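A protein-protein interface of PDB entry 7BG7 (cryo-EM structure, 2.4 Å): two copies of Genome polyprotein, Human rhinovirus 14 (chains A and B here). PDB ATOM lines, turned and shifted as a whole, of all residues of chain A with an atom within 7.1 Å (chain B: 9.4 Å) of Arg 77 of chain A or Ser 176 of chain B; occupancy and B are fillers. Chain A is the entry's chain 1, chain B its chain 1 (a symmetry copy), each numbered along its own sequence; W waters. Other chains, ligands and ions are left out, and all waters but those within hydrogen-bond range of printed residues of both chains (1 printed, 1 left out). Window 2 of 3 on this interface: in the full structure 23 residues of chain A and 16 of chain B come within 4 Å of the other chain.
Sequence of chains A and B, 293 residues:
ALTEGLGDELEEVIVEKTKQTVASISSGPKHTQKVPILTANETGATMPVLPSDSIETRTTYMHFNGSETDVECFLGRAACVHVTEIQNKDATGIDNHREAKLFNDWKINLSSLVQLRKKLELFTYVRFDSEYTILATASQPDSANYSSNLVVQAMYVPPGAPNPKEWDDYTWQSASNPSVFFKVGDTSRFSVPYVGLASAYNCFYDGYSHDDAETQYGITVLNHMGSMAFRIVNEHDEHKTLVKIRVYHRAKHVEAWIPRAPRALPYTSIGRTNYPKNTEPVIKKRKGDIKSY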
ATOM      1  N   GLU A  68      22.716 -14.606 -17.373  1.00  0.00           N
ATOM      2  CA  GLU A  68      22.278 -14.877 -16.015  1.00  0.00           C
ATOM      3  C   GLU A  68      23.097 -15.977 -15.357  1.00  0.00           C
ATOM      4  O   GLU A  68      22.879 -16.276 -14.182  1.00  0.00           O
ATOM      5  CB  GLU A  68      20.802 -15.251 -16.011  1.00  0.00           C
ATOM      6  CG  GLU A  68      20.003 -14.503 -14.976  1.00  0.00           C
ATOM      7  CD  GLU A  68      18.549 -14.896 -14.973  1.00  0.00           C
ATOM      8  OE1 GLU A  68      18.000 -15.148 -13.886  1.00  0.00           O
ATOM      9  OE2 GLU A  68      17.953 -14.972 -16.063  1.00  0.00           O
ATOM     10  N   GLU A  72      28.947 -12.878 -12.056  1.00  0.00           N
ATOM     11  CA  GLU A  72      28.505 -11.602 -11.507  1.00  0.00           C
ATOM     12  C   GLU A  72      27.022 -11.653 -11.178  1.00  0.00           C
ATOM     13  O   GLU A  72      26.584 -11.083 -10.178  1.00  0.00           O
ATOM     14  CB  GLU A  72      28.792 -10.465 -12.490  1.00  0.00           C
ATOM     15  CG  GLU A  72      28.370  -9.069 -12.009  1.00  0.00           C
ATOM     16  CD  GLU A  72      29.429  -8.342 -11.207  1.00  0.00           C
ATOM     17  OE1 GLU A  72      29.163  -8.007 -10.038  1.00  0.00           O
ATOM     18  OE2 GLU A  72      30.515  -8.082 -11.755  1.00  0.00           O
ATOM     19  N   CYS A  73      26.235 -12.333 -12.003  1.00  0.00           N
ATOM     20  CA  CYS A  73      24.808 -12.438 -11.741  1.00  0.00           C
ATOM     21  C   CYS A  73      24.494 -13.606 -10.818  1.00  0.00           C
ATOM     22  O   CYS A  73      23.635 -13.485  -9.941  1.00  0.00           O
ATOM     23  CB  CYS A  73      24.035 -12.596 -13.055  1.00  0.00           C
ATOM     24  SG  CYS A  73      22.245 -12.408 -12.892  1.00  0.00           S
ATOM     25  N   PHE A  74      25.184 -14.728 -10.997  1.00  0.00           N
ATOM     26  CA  PHE A  74      24.911 -15.918 -10.199  1.00  0.00           C
ATOM     27  C   PHE A  74      25.112 -15.645  -8.714  1.00  0.00           C
ATOM     28  O   PHE A  74      24.338 -16.118  -7.877  1.00  0.00           O
ATOM     29  CB  PHE A  74      25.797 -17.062 -10.670  1.00  0.00           C
ATOM     30  CG  PHE A  74      25.621 -18.328  -9.892  1.00  0.00           C
ATOM     31  CD1 PHE A  74      24.477 -19.089 -10.027  1.00  0.00           C
ATOM     32  CD2 PHE A  74      26.607 -18.765  -9.028  1.00  0.00           C
ATOM     33  CE1 PHE A  74      24.318 -20.262  -9.317  1.00  0.00           C
ATOM     34  CE2 PHE A  74      26.454 -19.935  -8.314  1.00  0.00           C
ATOM     35  CZ  PHE A  74      25.306 -20.684  -8.459  1.00  0.00           C
ATOM     36  N   LEU A  75      26.130 -14.867  -8.368  1.00  0.00           N
ATOM     37  CA  LEU A  75      26.469 -14.558  -6.986  1.00  0.00           C
ATOM     38  C   LEU A  75      26.155 -13.107  -6.638  1.00  0.00           C
ATOM     39  O   LEU A  75      26.752 -12.548  -5.722  1.00  0.00           O
ATOM     40  CB  LEU A  75      27.954 -14.814  -6.739  1.00  0.00           C
ATOM     41  CG  LEU A  75      28.530 -16.208  -6.943  1.00  0.00           C
ATOM     42  CD1 LEU A  75      30.042 -16.113  -7.064  1.00  0.00           C
ATOM     43  CD2 LEU A  75      28.135 -17.103  -5.797  1.00  0.00           C
ATOM     44  N   GLY A  76      25.201 -12.497  -7.334  1.00  0.00           N
ATOM     45  CA  GLY A  76      25.124 -11.052  -7.373  1.00  0.00           C
ATOM     46  C   GLY A  76      23.791 -10.389  -7.105  1.00  0.00           C
ATOM     47  O   GLY A  76      23.456  -9.410  -7.780  1.00  0.00           O
ATOM     48  N   ARG A  77      23.018 -10.879  -6.146  1.00  0.00           N
ATOM     49  CA  ARG A  77      21.874 -10.127  -5.656  1.00  0.00           C
ATOM     50  C   ARG A  77      21.934 -10.037  -4.139  1.00  0.00           C
ATOM     51  O   ARG A  77      22.633 -10.804  -3.476  1.00  0.00           O
ATOM     52  CB  ARG A  77      20.549 -10.726  -6.127  1.00  0.00           C
ATOM     53  CG  ARG A  77      20.381 -12.209  -5.925  1.00  0.00           C
ATOM     54  CD  ARG A  77      19.075 -12.654  -6.560  1.00  0.00           C
ATOM     55  NE  ARG A  77      19.044 -12.307  -7.977  1.00  0.00           N
ATOM     56  CZ  ARG A  77      18.013 -12.502  -8.794  1.00  0.00           C
ATOM     57  NH1 ARG A  77      16.892 -13.046  -8.355  1.00  0.00           N
ATOM     58  NH2 ARG A  77      18.115 -12.150 -10.067  1.00  0.00           N
ATOM     59  N   ALA A  78      21.209  -9.065  -3.601  1.00  0.00           N
ATOM     60  CA  ALA A  78      21.287  -8.774  -2.180  1.00  0.00           C
ATOM     61  C   ALA A  78      20.636  -9.884  -1.369  1.00  0.00           C
ATOM     62  O   ALA A  78      19.508 -10.297  -1.649  1.00  0.00           O
ATOM     63  CB  ALA A  78      20.623  -7.431  -1.880  1.00  0.00           C
ATOM     64  N   ALA A  79      21.353 -10.359  -0.357  1.00  0.00           N
ATOM     65  CA  ALA A  79      20.875 -11.405   0.532  1.00  0.00           C
ATOM     66  C   ALA A  79      21.077 -10.970   1.972  1.00  0.00           C
ATOM     67  O   ALA A  79      22.098 -10.365   2.309  1.00  0.00           O
ATOM     68  CB  ALA A  79      21.607 -12.722   0.273  1.00  0.00           C
ATOM     69  N   CYS A  80      20.101 -11.288   2.812  1.00  0.00           N
ATOM     70  CA  CYS A  80      20.184 -11.000   4.236  1.00  0.00           C
ATOM     71  C   CYS A  80      21.230 -11.889   4.886  1.00  0.00           C
ATOM     72  O   CYS A  80      21.099 -13.116   4.885  1.00  0.00           O
ATOM     73  CB  CYS A  80      18.831 -11.198   4.909  1.00  0.00           C
ATOM     74  SG  CYS A  80      18.844 -10.932   6.707  1.00  0.00           S
ATOM     75  N   GLN A 115      22.274 -20.658   1.849  1.00  0.00           N
ATOM     76  CA  GLN A 115      22.101 -20.511   0.406  1.00  0.00           C
ATOM     77  C   GLN A 115      23.299 -19.773  -0.185  1.00  0.00           C
ATOM     78  O   GLN A 115      23.964 -20.251  -1.121  1.00  0.00           O
ATOM     79  CB  GLN A 115      20.805 -19.754   0.116  1.00  0.00           C
ATOM     80  CG  GLN A 115      19.541 -20.548   0.395  1.00  0.00           C
ATOM     81  CD  GLN A 115      19.323 -21.697  -0.564  1.00  0.00           C
ATOM     82  OE1 GLN A 115      19.736 -21.646  -1.718  1.00  0.00           O
ATOM     83  NE2 GLN A 115      18.668 -22.743  -0.087  1.00  0.00           N
ATOM     84  N   LEU A 116      23.616 -18.621   0.398  1.00  0.00           N
ATOM     85  CA  LEU A 116      24.729 -17.827  -0.082  1.00  0.00           C
ATOM     86  C   LEU A 116      26.037 -18.571   0.122  1.00  0.00           C
ATOM     87  O   LEU A 116      26.922 -18.532  -0.738  1.00  0.00           O
ATOM     88  CB  LEU A 116      24.745 -16.488   0.649  1.00  0.00           C
ATOM     89  CG  LEU A 116      25.857 -15.524   0.273  1.00  0.00           C
ATOM     90  CD1 LEU A 116      25.814 -15.239  -1.212  1.00  0.00           C
ATOM     91  CD2 LEU A 116      25.736 -14.249   1.080  1.00  0.00           C
ATOM     92  N   LYS A 119      26.529 -21.215  -2.531  1.00  0.00           N
ATOM     93  CA  LYS A 119      26.816 -20.610  -3.826  1.00  0.00           C
ATOM     94  C   LYS A 119      28.264 -20.147  -3.872  1.00  0.00           C
ATOM     95  O   LYS A 119      28.974 -20.389  -4.851  1.00  0.00           O
ATOM     96  CB  LYS A 119      25.857 -19.451  -4.102  1.00  0.00           C
ATOM     97  CG  LYS A 119      24.534 -19.890  -4.684  1.00  0.00           C
ATOM     98  CD  LYS A 119      23.832 -18.784  -5.455  1.00  0.00           C
ATOM     99  CE  LYS A 119      23.229 -17.754  -4.535  1.00  0.00           C
ATOM    100  NZ  LYS A 119      22.393 -16.787  -5.295  1.00  0.00           N
ATOM    101  N   HIS A 249      23.718  -8.081   2.078  1.00  0.00           N
ATOM    102  CA  HIS A 249      24.967  -7.975   1.350  1.00  0.00           C
ATOM    103  C   HIS A 249      24.721  -8.310  -0.111  1.00  0.00           C
ATOM    104  O   HIS A 249      24.008  -9.262  -0.430  1.00  0.00           O
ATOM    105  CB  HIS A 249      26.028  -8.912   1.925  1.00  0.00           C
ATOM    106  CG  HIS A 249      27.300  -8.922   1.143  1.00  0.00           C
ATOM    107  ND1 HIS A 249      27.480  -9.706   0.027  1.00  0.00           N
ATOM    108  CD2 HIS A 249      28.454  -8.239   1.313  1.00  0.00           C
ATOM    109  CE1 HIS A 249      28.688  -9.499  -0.461  1.00  0.00           C
ATOM    110  NE2 HIS A 249      29.300  -8.616   0.303  1.00  0.00           N
ATOM    111  N   ARG A 250      25.284  -7.500  -0.995  1.00  0.00           N
ATOM    112  CA  ARG A 250      25.278  -7.776  -2.420  1.00  0.00           C
ATOM    113  C   ARG A 250      26.707  -7.704  -2.919  1.00  0.00           C
ATOM    114  O   ARG A 250      27.367  -6.671  -2.774  1.00  0.00           O
ATOM    115  CB  ARG A 250      24.382  -6.803  -3.181  1.00  0.00           C
ATOM    116  CG  ARG A 250      24.233  -7.153  -4.646  1.00  0.00           C
ATOM    117  CD  ARG A 250      23.219  -6.254  -5.322  1.00  0.00           C
ATOM    118  NE  ARG A 250      23.718  -4.897  -5.513  1.00  0.00           N
ATOM    119  CZ  ARG A 250      24.466  -4.505  -6.539  1.00  0.00           C
ATOM    120  NH1 ARG A 250      24.817  -5.360  -7.485  1.00  0.00           N
ATOM    121  NH2 ARG A 250      24.863  -3.248  -6.617  1.00  0.00           N
ATOM    122  N   ALA A 251      27.194  -8.811  -3.456  1.00  0.00           N
ATOM    123  CA  ALA A 251      28.517  -8.862  -4.051  1.00  0.00           C
ATOM    124  C   ALA A 251      28.470  -8.298  -5.464  1.00  0.00           C
ATOM    125  O   ALA A 251      27.562  -8.615  -6.236  1.00  0.00           O
ATOM    126  CB  ALA A 251      29.030 -10.299  -4.066  1.00  0.00           C
ATOM    127  N   MET B 155       7.740 -10.720  -2.018  1.00  0.00           N
ATOM    128  CA  MET B 155       8.734 -11.615  -2.579  1.00  0.00           C
ATOM    129  C   MET B 155       8.172 -12.270  -3.828  1.00  0.00           C
ATOM    130  O   MET B 155       7.200 -13.025  -3.758  1.00  0.00           O
ATOM    131  CB  MET B 155       9.146 -12.675  -1.561  1.00  0.00           C
ATOM    132  CG  MET B 155      10.311 -13.547  -2.010  1.00  0.00           C
ATOM    133  SD  MET B 155      11.076 -14.452  -0.656  1.00  0.00           S
ATOM    134  CE  MET B 155       9.752 -15.565  -0.235  1.00  0.00           C
ATOM    135  N   TYR B 156       8.783 -11.974  -4.962  1.00  0.00           N
ATOM    136  CA  TYR B 156       8.500 -12.697  -6.187  1.00  0.00           C
ATOM    137  C   TYR B 156       9.223 -14.033  -6.133  1.00  0.00           C
ATOM    138  O   TYR B 156      10.454 -14.070  -6.071  1.00  0.00           O
ATOM    139  CB  TYR B 156       8.942 -11.891  -7.401  1.00  0.00           C
ATOM    140  CG  TYR B 156       8.782 -12.628  -8.702  1.00  0.00           C
ATOM    141  CD1 TYR B 156       7.635 -12.489  -9.466  1.00  0.00           C
ATOM    142  CD2 TYR B 156       9.774 -13.472  -9.164  1.00  0.00           C
ATOM    143  CE1 TYR B 156       7.490 -13.160 -10.654  1.00  0.00           C
ATOM    144  CE2 TYR B 156       9.636 -14.152 -10.348  1.00  0.00           C
ATOM    145  CZ  TYR B 156       8.490 -13.996 -11.089  1.00  0.00           C
ATOM    146  OH  TYR B 156       8.356 -14.671 -12.274  1.00  0.00           O
ATOM    147  N   VAL B 157       8.474 -15.122  -6.108  1.00  0.00           N
ATOM    148  CA  VAL B 157       9.041 -16.467  -6.152  1.00  0.00           C
ATOM    149  C   VAL B 157       8.949 -16.972  -7.589  1.00  0.00           C
ATOM    150  O   VAL B 157       7.869 -16.887  -8.189  1.00  0.00           O
ATOM    151  CB  VAL B 157       8.328 -17.428  -5.183  1.00  0.00           C
ATOM    152  CG1 VAL B 157       8.147 -16.784  -3.825  1.00  0.00           C
ATOM    153  CG2 VAL B 157       7.035 -17.835  -5.726  1.00  0.00           C
ATOM    154  N   PRO B 158      10.039 -17.453  -8.181  1.00  0.00           N
ATOM    155  CA  PRO B 158       9.979 -18.005  -9.541  1.00  0.00           C
ATOM    156  C   PRO B 158       8.993 -19.155  -9.643  1.00  0.00           C
ATOM    157  O   PRO B 158       8.701 -19.820  -8.639  1.00  0.00           O
ATOM    158  CB  PRO B 158      11.417 -18.483  -9.784  1.00  0.00           C
ATOM    159  CG  PRO B 158      12.232 -17.647  -8.897  1.00  0.00           C
ATOM    160  CD  PRO B 158      11.418 -17.465  -7.664  1.00  0.00           C
ATOM    161  N   ALA B 161       8.939 -22.486  -7.392  1.00  0.00           N
ATOM    162  CA  ALA B 161       9.799 -22.360  -6.232  1.00  0.00           C
ATOM    163  C   ALA B 161       8.972 -22.468  -4.951  1.00  0.00           C
ATOM    164  O   ALA B 161       7.781 -22.149  -4.943  1.00  0.00           O
ATOM    165  CB  ALA B 161      10.547 -21.031  -6.263  1.00  0.00           C
ATOM    166  N   TYR B 170      12.757 -19.230   6.722  1.00  0.00           N
ATOM    167  CA  TYR B 170      13.989 -18.831   6.056  1.00  0.00           C
ATOM    168  C   TYR B 170      13.792 -18.633   4.563  1.00  0.00           C
ATOM    169  O   TYR B 170      14.693 -18.113   3.904  1.00  0.00           O
ATOM    170  CB  TYR B 170      15.104 -19.847   6.298  1.00  0.00           C
ATOM    171  CG  TYR B 170      15.925 -19.523   7.518  1.00  0.00           C
ATOM    172  CD1 TYR B 170      15.675 -20.143   8.732  1.00  0.00           C
ATOM    173  CD2 TYR B 170      16.931 -18.577   7.462  1.00  0.00           C
ATOM    174  CE1 TYR B 170      16.416 -19.836   9.848  1.00  0.00           C
ATOM    175  CE2 TYR B 170      17.674 -18.262   8.572  1.00  0.00           C
ATOM    176  CZ  TYR B 170      17.413 -18.892   9.763  1.00  0.00           C
ATOM    177  OH  TYR B 170      18.157 -18.583  10.870  1.00  0.00           O
ATOM    178  N   THR B 171      12.641 -19.035   4.022  1.00  0.00           N
ATOM    179  CA  THR B 171      12.360 -18.796   2.613  1.00  0.00           C
ATOM    180  C   THR B 171      12.339 -17.309   2.308  1.00  0.00           C
ATOM    181  O   THR B 171      12.652 -16.900   1.187  1.00  0.00           O
ATOM    182  CB  THR B 171      11.029 -19.435   2.221  1.00  0.00           C
ATOM    183  OG1 THR B 171      11.062 -20.835   2.522  1.00  0.00           O
ATOM    184  CG2 THR B 171      10.763 -19.241   0.742  1.00  0.00           C
ATOM    185  N   TRP B 172      11.971 -16.485   3.291  1.00  0.00           N
ATOM    186  CA  TRP B 172      11.937 -15.045   3.085  1.00  0.00           C
ATOM    187  C   TRP B 172      13.340 -14.486   2.909  1.00  0.00           C
ATOM    188  O   TRP B 172      13.511 -13.447   2.263  1.00  0.00           O
ATOM    189  CB  TRP B 172      11.232 -14.367   4.250  1.00  0.00           C
ATOM    190  CG  TRP B 172       9.816 -14.788   4.423  1.00  0.00           C
ATOM    191  CD1 TRP B 172       9.341 -15.685   5.322  1.00  0.00           C
ATOM    192  CD2 TRP B 172       8.681 -14.300   3.702  1.00  0.00           C
ATOM    193  NE1 TRP B 172       7.982 -15.801   5.199  1.00  0.00           N
ATOM    194  CE2 TRP B 172       7.551 -14.958   4.212  1.00  0.00           C
ATOM    195  CE3 TRP B 172       8.510 -13.373   2.668  1.00  0.00           C
ATOM    196  CZ2 TRP B 172       6.272 -14.722   3.727  1.00  0.00           C
ATOM    197  CZ3 TRP B 172       7.237 -13.141   2.192  1.00  0.00           C
ATOM    198  CH2 TRP B 172       6.136 -13.815   2.718  1.00  0.00           C
ATOM    199  N   GLN B 173      14.348 -15.148   3.476  1.00  0.00           N
ATOM    200  CA  GLN B 173      15.729 -14.698   3.377  1.00  0.00           C
ATOM    201  C   GLN B 173      16.428 -15.344   2.194  1.00  0.00           C
ATOM    202  O   GLN B 173      17.644 -15.551   2.219  1.00  0.00           O
ATOM    203  CB  GLN B 173      16.491 -15.010   4.666  1.00  0.00           C
ATOM    204  CG  GLN B 173      15.732 -14.741   5.948  1.00  0.00           C
ATOM    205  CD  GLN B 173      15.147 -13.349   6.008  1.00  0.00           C
ATOM    206  OE1 GLN B 173      13.974 -13.175   6.312  1.00  0.00           O
ATOM    207  NE2 GLN B 173      15.968 -12.347   5.722  1.00  0.00           N
ATOM    208  N   SER B 174      15.658 -15.681   1.166  1.00  0.00           N
ATOM    209  CA  SER B 174      16.172 -16.325  -0.032  1.00  0.00           C
ATOM    210  C   SER B 174      17.223 -15.460  -0.712  1.00  0.00           C
ATOM    211  O   SER B 174      17.000 -14.277  -0.975  1.00  0.00           O
ATOM    212  CB  SER B 174      15.025 -16.621  -0.994  1.00  0.00           C
ATOM    213  OG  SER B 174      15.504 -17.188  -2.198  1.00  0.00           O
ATOM    214  N   ALA B 175      18.366 -16.059  -1.011  1.00  0.00           N
ATOM    215  CA  ALA B 175      19.453 -15.343  -1.655  1.00  0.00           C
ATOM    216  C   ALA B 175      19.210 -15.163  -3.146  1.00  0.00           C
ATOM    217  O   ALA B 175      20.048 -14.562  -3.825  1.00  0.00           O
ATOM    218  CB  ALA B 175      20.781 -16.072  -1.427  1.00  0.00           C
ATOM    219  N   SER B 176      18.101 -15.678  -3.670  1.00  0.00           N
ATOM    220  CA  SER B 176      17.816 -15.687  -5.101  1.00  0.00           C
ATOM    221  C   SER B 176      16.465 -15.073  -5.436  1.00  0.00           C
ATOM    222  O   SER B 176      16.340 -14.433  -6.477  1.00  0.00           O
ATOM    223  CB  SER B 176      17.875 -17.115  -5.659  1.00  0.00           C
ATOM    224  OG  SER B 176      19.215 -17.559  -5.784  1.00  0.00           O
ATOM    225  N   ASN B 177      15.456 -15.255  -4.591  1.00  0.00           N
ATOM    226  CA  ASN B 177      14.131 -14.716  -4.894  1.00  0.00           C
ATOM    227  C   ASN B 177      14.167 -13.192  -4.851  1.00  0.00           C
ATOM    228  O   ASN B 177      14.607 -12.618  -3.851  1.00  0.00           O
ATOM    229  CB  ASN B 177      13.088 -15.224  -3.904  1.00  0.00           C
ATOM    230  CG  ASN B 177      12.898 -16.721  -3.965  1.00  0.00           C
ATOM    231  OD1 ASN B 177      13.182 -17.358  -4.971  1.00  0.00           O
ATOM    232  ND2 ASN B 177      12.426 -17.290  -2.872  1.00  0.00           N
ATOM    233  N   PRO B 178      13.728 -12.503  -5.902  1.00  0.00           N
ATOM    234  CA  PRO B 178      13.613 -11.041  -5.826  1.00  0.00           C
ATOM    235  C   PRO B 178      12.625 -10.629  -4.745  1.00  0.00           C
ATOM    236  O   PRO B 178      11.523 -11.168  -4.652  1.00  0.00           O
ATOM    237  CB  PRO B 178      13.119 -10.647  -7.221  1.00  0.00           C
ATOM    238  CG  PRO B 178      13.480 -11.777  -8.083  1.00  0.00           C
ATOM    239  CD  PRO B 178      13.378 -12.997  -7.242  1.00  0.00           C
ATOM    240  N   SER B 179      13.033  -9.678  -3.917  1.00  0.00           N
ATOM    241  CA  SER B 179      12.186  -9.150  -2.860  1.00  0.00           C
ATOM    242  C   SER B 179      12.268  -7.636  -2.844  1.00  0.00           C
ATOM    243  O   SER B 179      13.313  -7.057  -3.148  1.00  0.00           O
ATOM    244  CB  SER B 179      12.570  -9.696  -1.491  1.00  0.00           C
ATOM    245  OG  SER B 179      12.259 -11.068  -1.400  1.00  0.00           O
ATOM    246  N   PRO B 193      10.391  -9.286 -16.724  1.00  0.00           N
ATOM    247  CA  PRO B 193      10.350  -9.567 -18.157  1.00  0.00           C
ATOM    248  C   PRO B 193       9.367 -10.689 -18.456  1.00  0.00           C
ATOM    249  O   PRO B 193       8.852 -11.363 -17.567  1.00  0.00           O
ATOM    250  CB  PRO B 193      11.788  -9.973 -18.490  1.00  0.00           C
ATOM    251  CG  PRO B 193      12.366 -10.419 -17.207  1.00  0.00           C
ATOM    252  CD  PRO B 193      11.707  -9.605 -16.144  1.00  0.00           C
HETATM  253  O   HOH W   1      18.228 -12.580   1.750  1.00  0.00           O
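NE2 of Gln 173 of chain B sits close to SG of Cys 80 of chain A, at 3.4 Å.
OG of Ser 176 of chain B lies within hydrogen-bond range of NZ of Lys 119 of chain A, 3.3 Å away.
The guanidinium group of Arg 77 of chain A sits close to the backbone carbonyl oxygen of Ser 176 of chain B (2.4 Å).
The backbone carbonyl oxygen (O) of Phe 74 of chain A is in hydrogen-bond range of the side-chain amino group (NZ) of Lys 119 of chain A, 3.3 Å away.
The backbone NH of His 249 of chain A sits at hydrogen-bond distance from the backbone carbonyl oxygen of Ala 79 of chain A, 2.8 Å away.
The backbone NH (N) of Tyr 156 of chain B is in hydrogen-bond range of the backbone carbonyl oxygen (O) of Pro 178 of chain B, at 2.9 Å.
The backbone NH (N) of Ser 176 of chain B sits close to the side-chain hydroxyl (OG) of Ser 174 of chain B, 3.3 Å away.
CG of Arg 77 of chain A touches O of Ala 175 of chain B, 3.2 Å away.
Arg 77 of chain A touches Pro 178 of chain B (NH1 to CG, 3.7 Å).
CB of Ala 79 of chain A touches CB of Ala 175 of chain B, 3.8 Å away.
Ala 175 of chain B touches Gln 115 of chain A.
Lys 119 of chain A touches Ala 175 of chain B (NZ to O, 3.6 Å).
No residue of chain B comes within 4 Å of Gly 76 of chain A.
Of chain B, only Ala 175 (3.2 Å), Ser 176 (2.4 Å) and Pro 178 (3.7 Å) come within 4 Å of Arg 77 of chain A.
No residue of chain B comes within 4 Å of Ala 78 of chain A.
Printed residues of chain B within 4 Å of Lys 119 of chain A: Ala 175 (3.6 Å) and Ser 176 (3.3 Å).
Of the printed residues of chain A, Gln 173 of chain B touches Cys 80 (3.2 Å).
Of chain A, only Arg 77 (2.4 Å) and Lys 119 (3.3 Å) come within 4 Å of Ser 176 of chain B.
The nearest residue of chain A that does not touch Ser 176 of chain B is Phe 74 of chain A (5.7 Å).
The nearest printed residue of chain B that does not touch Lys 119 of chain A is Ser 174 of chain B (7.0 Å).
Of the 16 printed residues of chain A, 5 touch a printed residue of chain B.
Printed residues of chain A that touch a printed residue of chain B: Arg 77, Ala 79, Cys 80, Gln 115 and Lys 119.
Hydrophobic or aromatic side chains of chain A within 4 Å of the printed part of chain B: Ala 79.
Along chain A the printed residues that touch a printed residue of chain B span positions 77 to 119.
Of the 16 printed residues of chain B, 4 touch a printed residue of chain A.
Hydrophobic or aromatic side chains of chain B within 4 Å of the printed part of chain A: Ala 175 and Pro 178.
Among the printed residues, no Asp or Glu carboxylate lies within 4 Å of a Lys or Arg side-chain nitrogen of the other chain.
No position is printed for both chains.
Water W1 lies within hydrogen-bond range of N of Cys 80 of chain A, O of Gln 173 of chain B and O of Ser 174 of chain B.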
